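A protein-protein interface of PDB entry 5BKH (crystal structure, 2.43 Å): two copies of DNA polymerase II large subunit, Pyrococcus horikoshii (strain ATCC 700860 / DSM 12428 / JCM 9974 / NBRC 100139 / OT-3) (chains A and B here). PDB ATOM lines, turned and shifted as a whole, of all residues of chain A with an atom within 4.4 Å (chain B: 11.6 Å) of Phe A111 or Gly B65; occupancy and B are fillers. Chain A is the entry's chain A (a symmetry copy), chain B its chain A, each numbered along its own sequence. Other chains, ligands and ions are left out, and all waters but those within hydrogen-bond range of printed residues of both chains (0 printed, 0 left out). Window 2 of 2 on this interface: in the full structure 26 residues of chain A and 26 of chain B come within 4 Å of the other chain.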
ATOM      1  N   LEU A 104      18.414  12.866 -13.710  1.00  0.00           N
ATOM      2  CA  LEU A 104      17.164  13.253 -14.352  1.00  0.00           C
ATOM      3  C   LEU A 104      17.434  13.690 -15.783  1.00  0.00           C
ATOM      4  O   LEU A 104      18.135  14.681 -16.017  1.00  0.00           O
ATOM      5  CB  LEU A 104      16.484  14.375 -13.580  1.00  0.00           C
ATOM      6  CG  LEU A 104      15.088  14.039 -13.062  1.00  0.00           C
ATOM      7  CD1 LEU A 104      14.290  15.316 -12.993  1.00  0.00           C
ATOM      8  CD2 LEU A 104      14.377  12.991 -13.924  1.00  0.00           C
ATOM      9  N   VAL A 105      16.859  12.967 -16.737  1.00  0.00           N
ATOM     10  CA  VAL A 105      17.096  13.174 -18.155  1.00  0.00           C
ATOM     11  C   VAL A 105      15.762  13.473 -18.819  1.00  0.00           C
ATOM     12  O   VAL A 105      14.722  12.952 -18.402  1.00  0.00           O
ATOM     13  CB  VAL A 105      17.780  11.935 -18.777  1.00  0.00           C
ATOM     14  CG1 VAL A 105      17.454  11.794 -20.255  1.00  0.00           C
ATOM     15  CG2 VAL A 105      19.279  12.015 -18.567  1.00  0.00           C
ATOM     16  N   TYR A 106      15.782  14.348 -19.819  1.00  0.00           N
ATOM     17  CA  TYR A 106      14.619  14.602 -20.658  1.00  0.00           C
ATOM     18  C   TYR A 106      14.825  13.896 -21.990  1.00  0.00           C
ATOM     19  O   TYR A 106      15.751  14.227 -22.735  1.00  0.00           O
ATOM     20  CB  TYR A 106      14.407  16.100 -20.871  1.00  0.00           C
ATOM     21  CG  TYR A 106      13.080  16.456 -21.501  1.00  0.00           C
ATOM     22  CD1 TYR A 106      11.927  16.542 -20.732  1.00  0.00           C
ATOM     23  CD2 TYR A 106      12.982  16.715 -22.868  1.00  0.00           C
ATOM     24  CE1 TYR A 106      10.710  16.870 -21.301  1.00  0.00           C
ATOM     25  CE2 TYR A 106      11.769  17.045 -23.447  1.00  0.00           C
ATOM     26  CZ  TYR A 106      10.637  17.123 -22.659  1.00  0.00           C
ATOM     27  OH  TYR A 106       9.430  17.453 -23.223  1.00  0.00           O
ATOM     28  N   LYS A 110       9.690  13.060 -22.099  1.00  0.00           N
ATOM     29  CA  LYS A 110       9.475  12.540 -20.759  1.00  0.00           C
ATOM     30  C   LYS A 110      10.683  12.824 -19.877  1.00  0.00           C
ATOM     31  O   LYS A 110      11.826  12.853 -20.344  1.00  0.00           O
ATOM     32  CB  LYS A 110       9.212  11.027 -20.778  1.00  0.00           C
ATOM     33  CG  LYS A 110       7.746  10.633 -20.799  1.00  0.00           C
ATOM     34  CD  LYS A 110       7.351  10.073 -22.158  1.00  0.00           C
ATOM     35  CE  LYS A 110       5.860   9.766 -22.225  1.00  0.00           C
ATOM     36  NZ  LYS A 110       5.278  10.127 -23.550  1.00  0.00           N
ATOM     37  N   PHE A 111      10.413  13.026 -18.590  1.00  0.00           N
ATOM     38  CA  PHE A 111      11.449  13.059 -17.568  1.00  0.00           C
ATOM     39  C   PHE A 111      11.654  11.642 -17.043  1.00  0.00           C
ATOM     40  O   PHE A 111      10.739  11.055 -16.458  1.00  0.00           O
ATOM     41  CB  PHE A 111      11.061  14.003 -16.433  1.00  0.00           C
ATOM     42  CG  PHE A 111      10.885  15.430 -16.866  1.00  0.00           C
ATOM     43  CD1 PHE A 111       9.705  15.844 -17.460  1.00  0.00           C
ATOM     44  CD2 PHE A 111      11.893  16.361 -16.672  1.00  0.00           C
ATOM     45  CE1 PHE A 111       9.534  17.158 -17.863  1.00  0.00           C
ATOM     46  CE2 PHE A 111      11.727  17.676 -17.070  1.00  0.00           C
ATOM     47  CZ  PHE A 111      10.544  18.075 -17.667  1.00  0.00           C
ATOM     48  N   VAL A 112      12.842  11.090 -17.266  1.00  0.00           N
ATOM     49  CA  VAL A 112      13.168   9.735 -16.845  1.00  0.00           C
ATOM     50  C   VAL A 112      14.414   9.761 -15.969  1.00  0.00           C
ATOM     51  O   VAL A 112      15.274  10.640 -16.085  1.00  0.00           O
ATOM     52  CB  VAL A 112      13.372   8.788 -18.050  1.00  0.00           C
ATOM     53  CG1 VAL A 112      12.294   9.001 -19.086  1.00  0.00           C
ATOM     54  CG2 VAL A 112      14.741   9.000 -18.675  1.00  0.00           C
ATOM     55  N   ILE A 126      18.108  17.810 -16.611  1.00  0.00           N
ATOM     56  CA  ILE A 126      17.319  18.830 -15.937  1.00  0.00           C
ATOM     57  C   ILE A 126      18.154  19.401 -14.799  1.00  0.00           C
ATOM     58  O   ILE A 126      18.626  18.658 -13.932  1.00  0.00           O
ATOM     59  CB  ILE A 126      15.995  18.257 -15.410  1.00  0.00           C
ATOM     60  CG1 ILE A 126      15.249  17.516 -16.520  1.00  0.00           C
ATOM     61  CG2 ILE A 126      15.139  19.366 -14.806  1.00  0.00           C
ATOM     62  CD1 ILE A 126      15.054  18.345 -17.786  1.00  0.00           C
ATOM     63  N   PRO A 135      13.052  24.847 -13.588  1.00  0.00           N
ATOM     64  CA  PRO A 135      13.755  23.725 -14.225  1.00  0.00           C
ATOM     65  C   PRO A 135      14.240  24.124 -15.613  1.00  0.00           C
ATOM     66  O   PRO A 135      13.477  24.645 -16.430  1.00  0.00           O
ATOM     67  CB  PRO A 135      12.696  22.618 -14.280  1.00  0.00           C
ATOM     68  CG  PRO A 135      11.390  23.327 -14.169  1.00  0.00           C
ATOM     69  CD  PRO A 135      11.634  24.550 -13.339  1.00  0.00           C
ATOM     70  N   LYS A 137      16.497  22.899 -19.125  1.00  0.00           N
ATOM     71  CA  LYS A 137      16.956  21.774 -19.933  1.00  0.00           C
ATOM     72  C   LYS A 137      18.309  22.133 -20.528  1.00  0.00           C
ATOM     73  O   LYS A 137      18.398  23.007 -21.394  1.00  0.00           O
ATOM     74  CB  LYS A 137      15.952  21.433 -21.031  1.00  0.00           C
ATOM     75  CG  LYS A 137      14.564  21.067 -20.521  1.00  0.00           C
ATOM     76  CD  LYS A 137      13.903  20.045 -21.419  1.00  0.00           C
ATOM     77  CE  LYS A 137      12.392  20.175 -21.386  1.00  0.00           C
ATOM     78  NZ  LYS A 137      11.860  20.479 -20.034  1.00  0.00           N
ATOM     79  N   SER B  59      11.851  19.941  -3.689  1.00  0.00           N
ATOM     80  CA  SER B  59      12.070  18.716  -4.443  1.00  0.00           C
ATOM     81  C   SER B  59      11.578  18.884  -5.880  1.00  0.00           C
ATOM     82  O   SER B  59      11.182  19.986  -6.282  1.00  0.00           O
ATOM     83  CB  SER B  59      11.361  17.549  -3.755  1.00  0.00           C
ATOM     84  OG  SER B  59      11.815  16.302  -4.243  1.00  0.00           O
ATOM     85  N   PHE B  60      11.569  17.798  -6.654  1.00  0.00           N
ATOM     86  CA  PHE B  60      11.185  17.844  -8.058  1.00  0.00           C
ATOM     87  C   PHE B  60      10.107  16.810  -8.347  1.00  0.00           C
ATOM     88  O   PHE B  60      10.182  15.672  -7.873  1.00  0.00           O
ATOM     89  CB  PHE B  60      12.393  17.596  -8.975  1.00  0.00           C
ATOM     90  CG  PHE B  60      12.143  17.946 -10.418  1.00  0.00           C
ATOM     91  CD1 PHE B  60      12.266  19.253 -10.859  1.00  0.00           C
ATOM     92  CD2 PHE B  60      11.780  16.970 -11.331  1.00  0.00           C
ATOM     93  CE1 PHE B  60      12.036  19.582 -12.179  1.00  0.00           C
ATOM     94  CE2 PHE B  60      11.548  17.292 -12.658  1.00  0.00           C
ATOM     95  CZ  PHE B  60      11.678  18.597 -13.081  1.00  0.00           C
ATOM     96  N   ASN B  61       9.106  17.214  -9.137  1.00  0.00           N
ATOM     97  CA  ASN B  61       8.035  16.346  -9.604  1.00  0.00           C
ATOM     98  C   ASN B  61       8.336  15.959 -11.042  1.00  0.00           C
ATOM     99  O   ASN B  61       8.149  16.782 -11.955  1.00  0.00           O
ATOM    100  CB  ASN B  61       6.683  17.060  -9.508  1.00  0.00           C
ATOM    101  CG  ASN B  61       5.508  16.112  -9.656  1.00  0.00           C
ATOM    102  OD1 ASN B  61       5.670  14.954 -10.042  1.00  0.00           O
ATOM    103  ND2 ASN B  61       4.313  16.604  -9.351  1.00  0.00           N
ATOM    104  N   PRO B  62       8.818  14.738 -11.302  1.00  0.00           N
ATOM    105  CA  PRO B  62       9.137  14.338 -12.678  1.00  0.00           C
ATOM    106  C   PRO B  62       7.926  13.968 -13.518  1.00  0.00           C
ATOM    107  O   PRO B  62       8.076  13.787 -14.733  1.00  0.00           O
ATOM    108  CB  PRO B  62      10.048  13.121 -12.478  1.00  0.00           C
ATOM    109  CG  PRO B  62       9.595  12.537 -11.190  1.00  0.00           C
ATOM    110  CD  PRO B  62       9.183  13.700 -10.323  1.00  0.00           C
ATOM    111  N   GLU B  63       6.744  13.834 -12.918  1.00  0.00           N
ATOM    112  CA  GLU B  63       5.543  13.581 -13.706  1.00  0.00           C
ATOM    113  C   GLU B  63       5.080  14.847 -14.416  1.00  0.00           C
ATOM    114  O   GLU B  63       4.804  14.826 -15.620  1.00  0.00           O
ATOM    115  CB  GLU B  63       4.433  13.023 -12.815  1.00  0.00           C
ATOM    116  CG  GLU B  63       4.572  11.539 -12.521  1.00  0.00           C
ATOM    117  CD  GLU B  63       5.504  11.258 -11.357  1.00  0.00           C
ATOM    118  OE1 GLU B  63       6.062  12.221 -10.789  1.00  0.00           O
ATOM    119  OE2 GLU B  63       5.682  10.072 -11.012  1.00  0.00           O
ATOM    120  N   GLU B  64       4.995  15.959 -13.685  1.00  0.00           N
ATOM    121  CA  GLU B  64       4.699  17.256 -14.278  1.00  0.00           C
ATOM    122  C   GLU B  64       5.952  18.055 -14.611  1.00  0.00           C
ATOM    123  O   GLU B  64       5.840  19.127 -15.217  1.00  0.00           O
ATOM    124  CB  GLU B  64       3.810  18.082 -13.340  1.00  0.00           C
ATOM    125  CG  GLU B  64       2.744  17.281 -12.611  1.00  0.00           C
ATOM    126  CD  GLU B  64       1.747  18.170 -11.892  1.00  0.00           C
ATOM    127  OE1 GLU B  64       1.402  19.241 -12.438  1.00  0.00           O
ATOM    128  OE2 GLU B  64       1.310  17.800 -10.781  1.00  0.00           O
ATOM    129  N   GLY B  65       7.130  17.563 -14.233  1.00  0.00           N
ATOM    130  CA  GLY B  65       8.371  18.274 -14.462  1.00  0.00           C
ATOM    131  C   GLY B  65       8.410  19.632 -13.794  1.00  0.00           C
ATOM    132  O   GLY B  65       8.763  20.630 -14.432  1.00  0.00           O
ATOM    133  N   LYS B  66       8.056  19.692 -12.509  1.00  0.00           N
ATOM    134  CA  LYS B  66       7.921  20.968 -11.818  1.00  0.00           C
ATOM    135  C   LYS B  66       8.638  20.938 -10.476  1.00  0.00           C
ATOM    136  O   LYS B  66       8.561  19.950  -9.741  1.00  0.00           O
ATOM    137  CB  LYS B  66       6.440  21.329 -11.603  1.00  0.00           C
ATOM    138  CG  LYS B  66       5.617  21.398 -12.887  1.00  0.00           C
ATOM    139  CD  LYS B  66       4.422  22.331 -12.747  1.00  0.00           C
ATOM    140  CE  LYS B  66       4.257  23.215 -13.978  1.00  0.00           C
ATOM    141  NZ  LYS B  66       3.932  24.627 -13.628  1.00  0.00           N
ATOM    142  N   VAL B  67       9.336  22.028 -10.158  1.00  0.00           N
ATOM    143  CA  VAL B  67       9.881  22.203  -8.818  1.00  0.00           C
ATOM    144  C   VAL B  67       8.732  22.355  -7.829  1.00  0.00           C
ATOM    145  O   VAL B  67       7.759  23.075  -8.090  1.00  0.00           O
ATOM    146  CB  VAL B  67      10.821  23.420  -8.778  1.00  0.00           C
ATOM    147  CG1 VAL B  67      11.281  23.697  -7.362  1.00  0.00           C
ATOM    148  CG2 VAL B  67      12.010  23.194  -9.697  1.00  0.00           C
ATOM    149  N   VAL B  68       8.833  21.673  -6.683  1.00  0.00           N
ATOM    150  CA  VAL B  68       7.724  21.585  -5.739  1.00  0.00           C
ATOM    151  C   VAL B  68       8.244  21.650  -4.306  1.00  0.00           C
ATOM    152  O   VAL B  68       9.419  21.403  -4.032  1.00  0.00           O
ATOM    153  CB  VAL B  68       6.904  20.292  -5.975  1.00  0.00           C
ATOM    154  CG1 VAL B  68       7.684  19.074  -5.519  1.00  0.00           C
ATOM    155  CG2 VAL B  68       5.534  20.373  -5.308  1.00  0.00           C
ATOM    156  N   LEU B  69       7.350  22.025  -3.389  1.00  0.00           N
ATOM    157  CA  LEU B  69       7.600  21.993  -1.952  1.00  0.00           C
ATOM    158  C   LEU B  69       7.077  20.703  -1.339  1.00  0.00           C
ATOM    159  O   LEU B  69       5.985  20.237  -1.683  1.00  0.00           O
ATOM    160  CB  LEU B  69       6.941  23.186  -1.259  1.00  0.00           C
ATOM    161  CG  LEU B  69       7.498  24.559  -1.618  1.00  0.00           C
ATOM    162  CD1 LEU B  69       6.642  25.637  -1.011  1.00  0.00           C
ATOM    163  CD2 LEU B  69       8.924  24.673  -1.067  1.00  0.00           C
ATOM    164  N   LYS B 160       6.541  11.988  -0.238  1.00  0.00           N
ATOM    165  CA  LYS B 160       6.313  11.806  -1.669  1.00  0.00           C
ATOM    166  C   LYS B 160       7.581  12.002  -2.497  1.00  0.00           C
ATOM    167  O   LYS B 160       8.158  11.030  -2.996  1.00  0.00           O
ATOM    168  CB  LYS B 160       5.213  12.752  -2.165  1.00  0.00           C
ATOM    169  CG  LYS B 160       4.323  12.161  -3.252  1.00  0.00           C
ATOM    170  CD  LYS B 160       3.128  13.059  -3.544  1.00  0.00           C
ATOM    171  CE  LYS B 160       2.488  12.722  -4.881  1.00  0.00           C
ATOM    172  NZ  LYS B 160       2.772  11.320  -5.299  1.00  0.00           N
ATOM    173  N   TYR B 161       8.019  13.246  -2.653  1.00  0.00           N
ATOM    174  CA  TYR B 161       9.140  13.579  -3.524  1.00  0.00           C
ATOM    175  C   TYR B 161      10.423  13.581  -2.702  1.00  0.00           C
ATOM    176  O   TYR B 161      10.623  14.457  -1.852  1.00  0.00           O
ATOM    177  CB  TYR B 161       8.899  14.928  -4.195  1.00  0.00           C
ATOM    178  CG  TYR B 161       7.532  15.033  -4.835  1.00  0.00           C
ATOM    179  CD1 TYR B 161       7.122  14.119  -5.800  1.00  0.00           C
ATOM    180  CD2 TYR B 161       6.640  16.024  -4.452  1.00  0.00           C
ATOM    181  CE1 TYR B 161       5.869  14.206  -6.382  1.00  0.00           C
ATOM    182  CE2 TYR B 161       5.386  16.122  -5.028  1.00  0.00           C
ATOM    183  CZ  TYR B 161       5.005  15.209  -5.991  1.00  0.00           C
ATOM    184  OH  TYR B 161       3.757  15.301  -6.564  1.00  0.00           O
ATOM    185  N   THR B 163      13.736  13.569  -3.805  1.00  0.00           N
ATOM    186  CA  THR B 163      14.956  14.131  -4.351  1.00  0.00           C
ATOM    187  C   THR B 163      15.230  15.493  -3.719  1.00  0.00           C
ATOM    188  O   THR B 163      14.356  16.113  -3.108  1.00  0.00           O
ATOM    189  CB  THR B 163      14.857  14.248  -5.870  1.00  0.00           C
ATOM    190  OG1 THR B 163      16.173  14.228  -6.429  1.00  0.00           O
ATOM    191  CG2 THR B 163      14.164  15.537  -6.260  1.00  0.00           C
ATOM    192  N   ILE B 165      17.693  19.316  -3.968  1.00  0.00           N
ATOM    193  CA  ILE B 165      18.306  20.257  -4.896  1.00  0.00           C
ATOM    194  C   ILE B 165      19.579  20.794  -4.263  1.00  0.00           C
ATOM    195  O   ILE B 165      19.537  21.580  -3.309  1.00  0.00           O
ATOM    196  CB  ILE B 165      17.342  21.387  -5.274  1.00  0.00           C
ATOM    197  CG1 ILE B 165      16.118  20.797  -5.976  1.00  0.00           C
ATOM    198  CG2 ILE B 165      18.039  22.395  -6.175  1.00  0.00           C
ATOM    199  CD1 ILE B 165      14.863  21.605  -5.795  1.00  0.00           C
ATOM    200  N   ILE B 170      19.750  18.127  -9.300  1.00  0.00           N
ATOM    201  CA  ILE B 170      18.704  17.333  -8.667  1.00  0.00           C
ATOM    202  C   ILE B 170      19.337  15.994  -8.302  1.00  0.00           C
ATOM    203  O   ILE B 170      19.550  15.144  -9.169  1.00  0.00           O
ATOM    204  CB  ILE B 170      17.501  17.155  -9.598  1.00  0.00           C
ATOM    205  CG1 ILE B 170      16.977  18.510 -10.073  1.00  0.00           C
ATOM    206  CG2 ILE B 170      16.408  16.341  -8.929  1.00  0.00           C
ATOM    207  CD1 ILE B 170      15.931  18.405 -11.175  1.00  0.00           C
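Among the printed residues, pairs that only touch across the chains: Leu A104 with Phe B60, Leu A104 with Ile B170, Phe A111 with Pro B62, Phe A111 with Gly B65, Ile A126 with Phe B60, Ile A126 with Ile B170, Pro A135 with Phe B60, Pro A135 with Gly B65 and Pro A135 with Val B67.
Of the printed residues of chain B, Leu A104 touches Phe B60 and Ile B170. Printed residues of chain B within 4 Å of Phe A111: Pro B62 and Gly B65. Val A112 touches none of the printed residues of chain B. Of the printed residues of chain A, Pro B62 touches Phe A111 (3.4 Å). Gly B65 touches just these residues of chain A: Phe A111 and Pro A135. Of the printed residues of chain A, Val B67 touches Pro A135 (3.9 Å). Val B68 touches none of the printed residues of chain A. The nearest printed residue of chain A that does not touch Gly B65 is Lys A137 (6.4 Å).
Of the 9 printed residues of chain A, 4 touch a printed residue of chain B. Hydrophobic or aromatic side chains of chain A that line the printed part of chain B: Leu A104, Phe A111, Ile A126 and Pro A135. Printed residues of chain B that touch a printed residue of chain A: Phe B60, Pro B62, Gly B65, Val B67 and Ile B170. Hydrophobic or aromatic side chains of chain B within 4 Å of the printed part of chain A: Phe B60, Val B67 and Ile B170. Among the printed residues, 9 pairs touch across the chains. Among the printed residues, no Asp or Glu carboxylate lies within 4 Å of a Lys or Arg side-chain nitrogen of the other chain.
No position is printed for both chains.
The backbone carbonyl oxygen of Leu A104 is in hydrogen-bond range of the backbone NH of Ile A126, 3.2 Å away.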
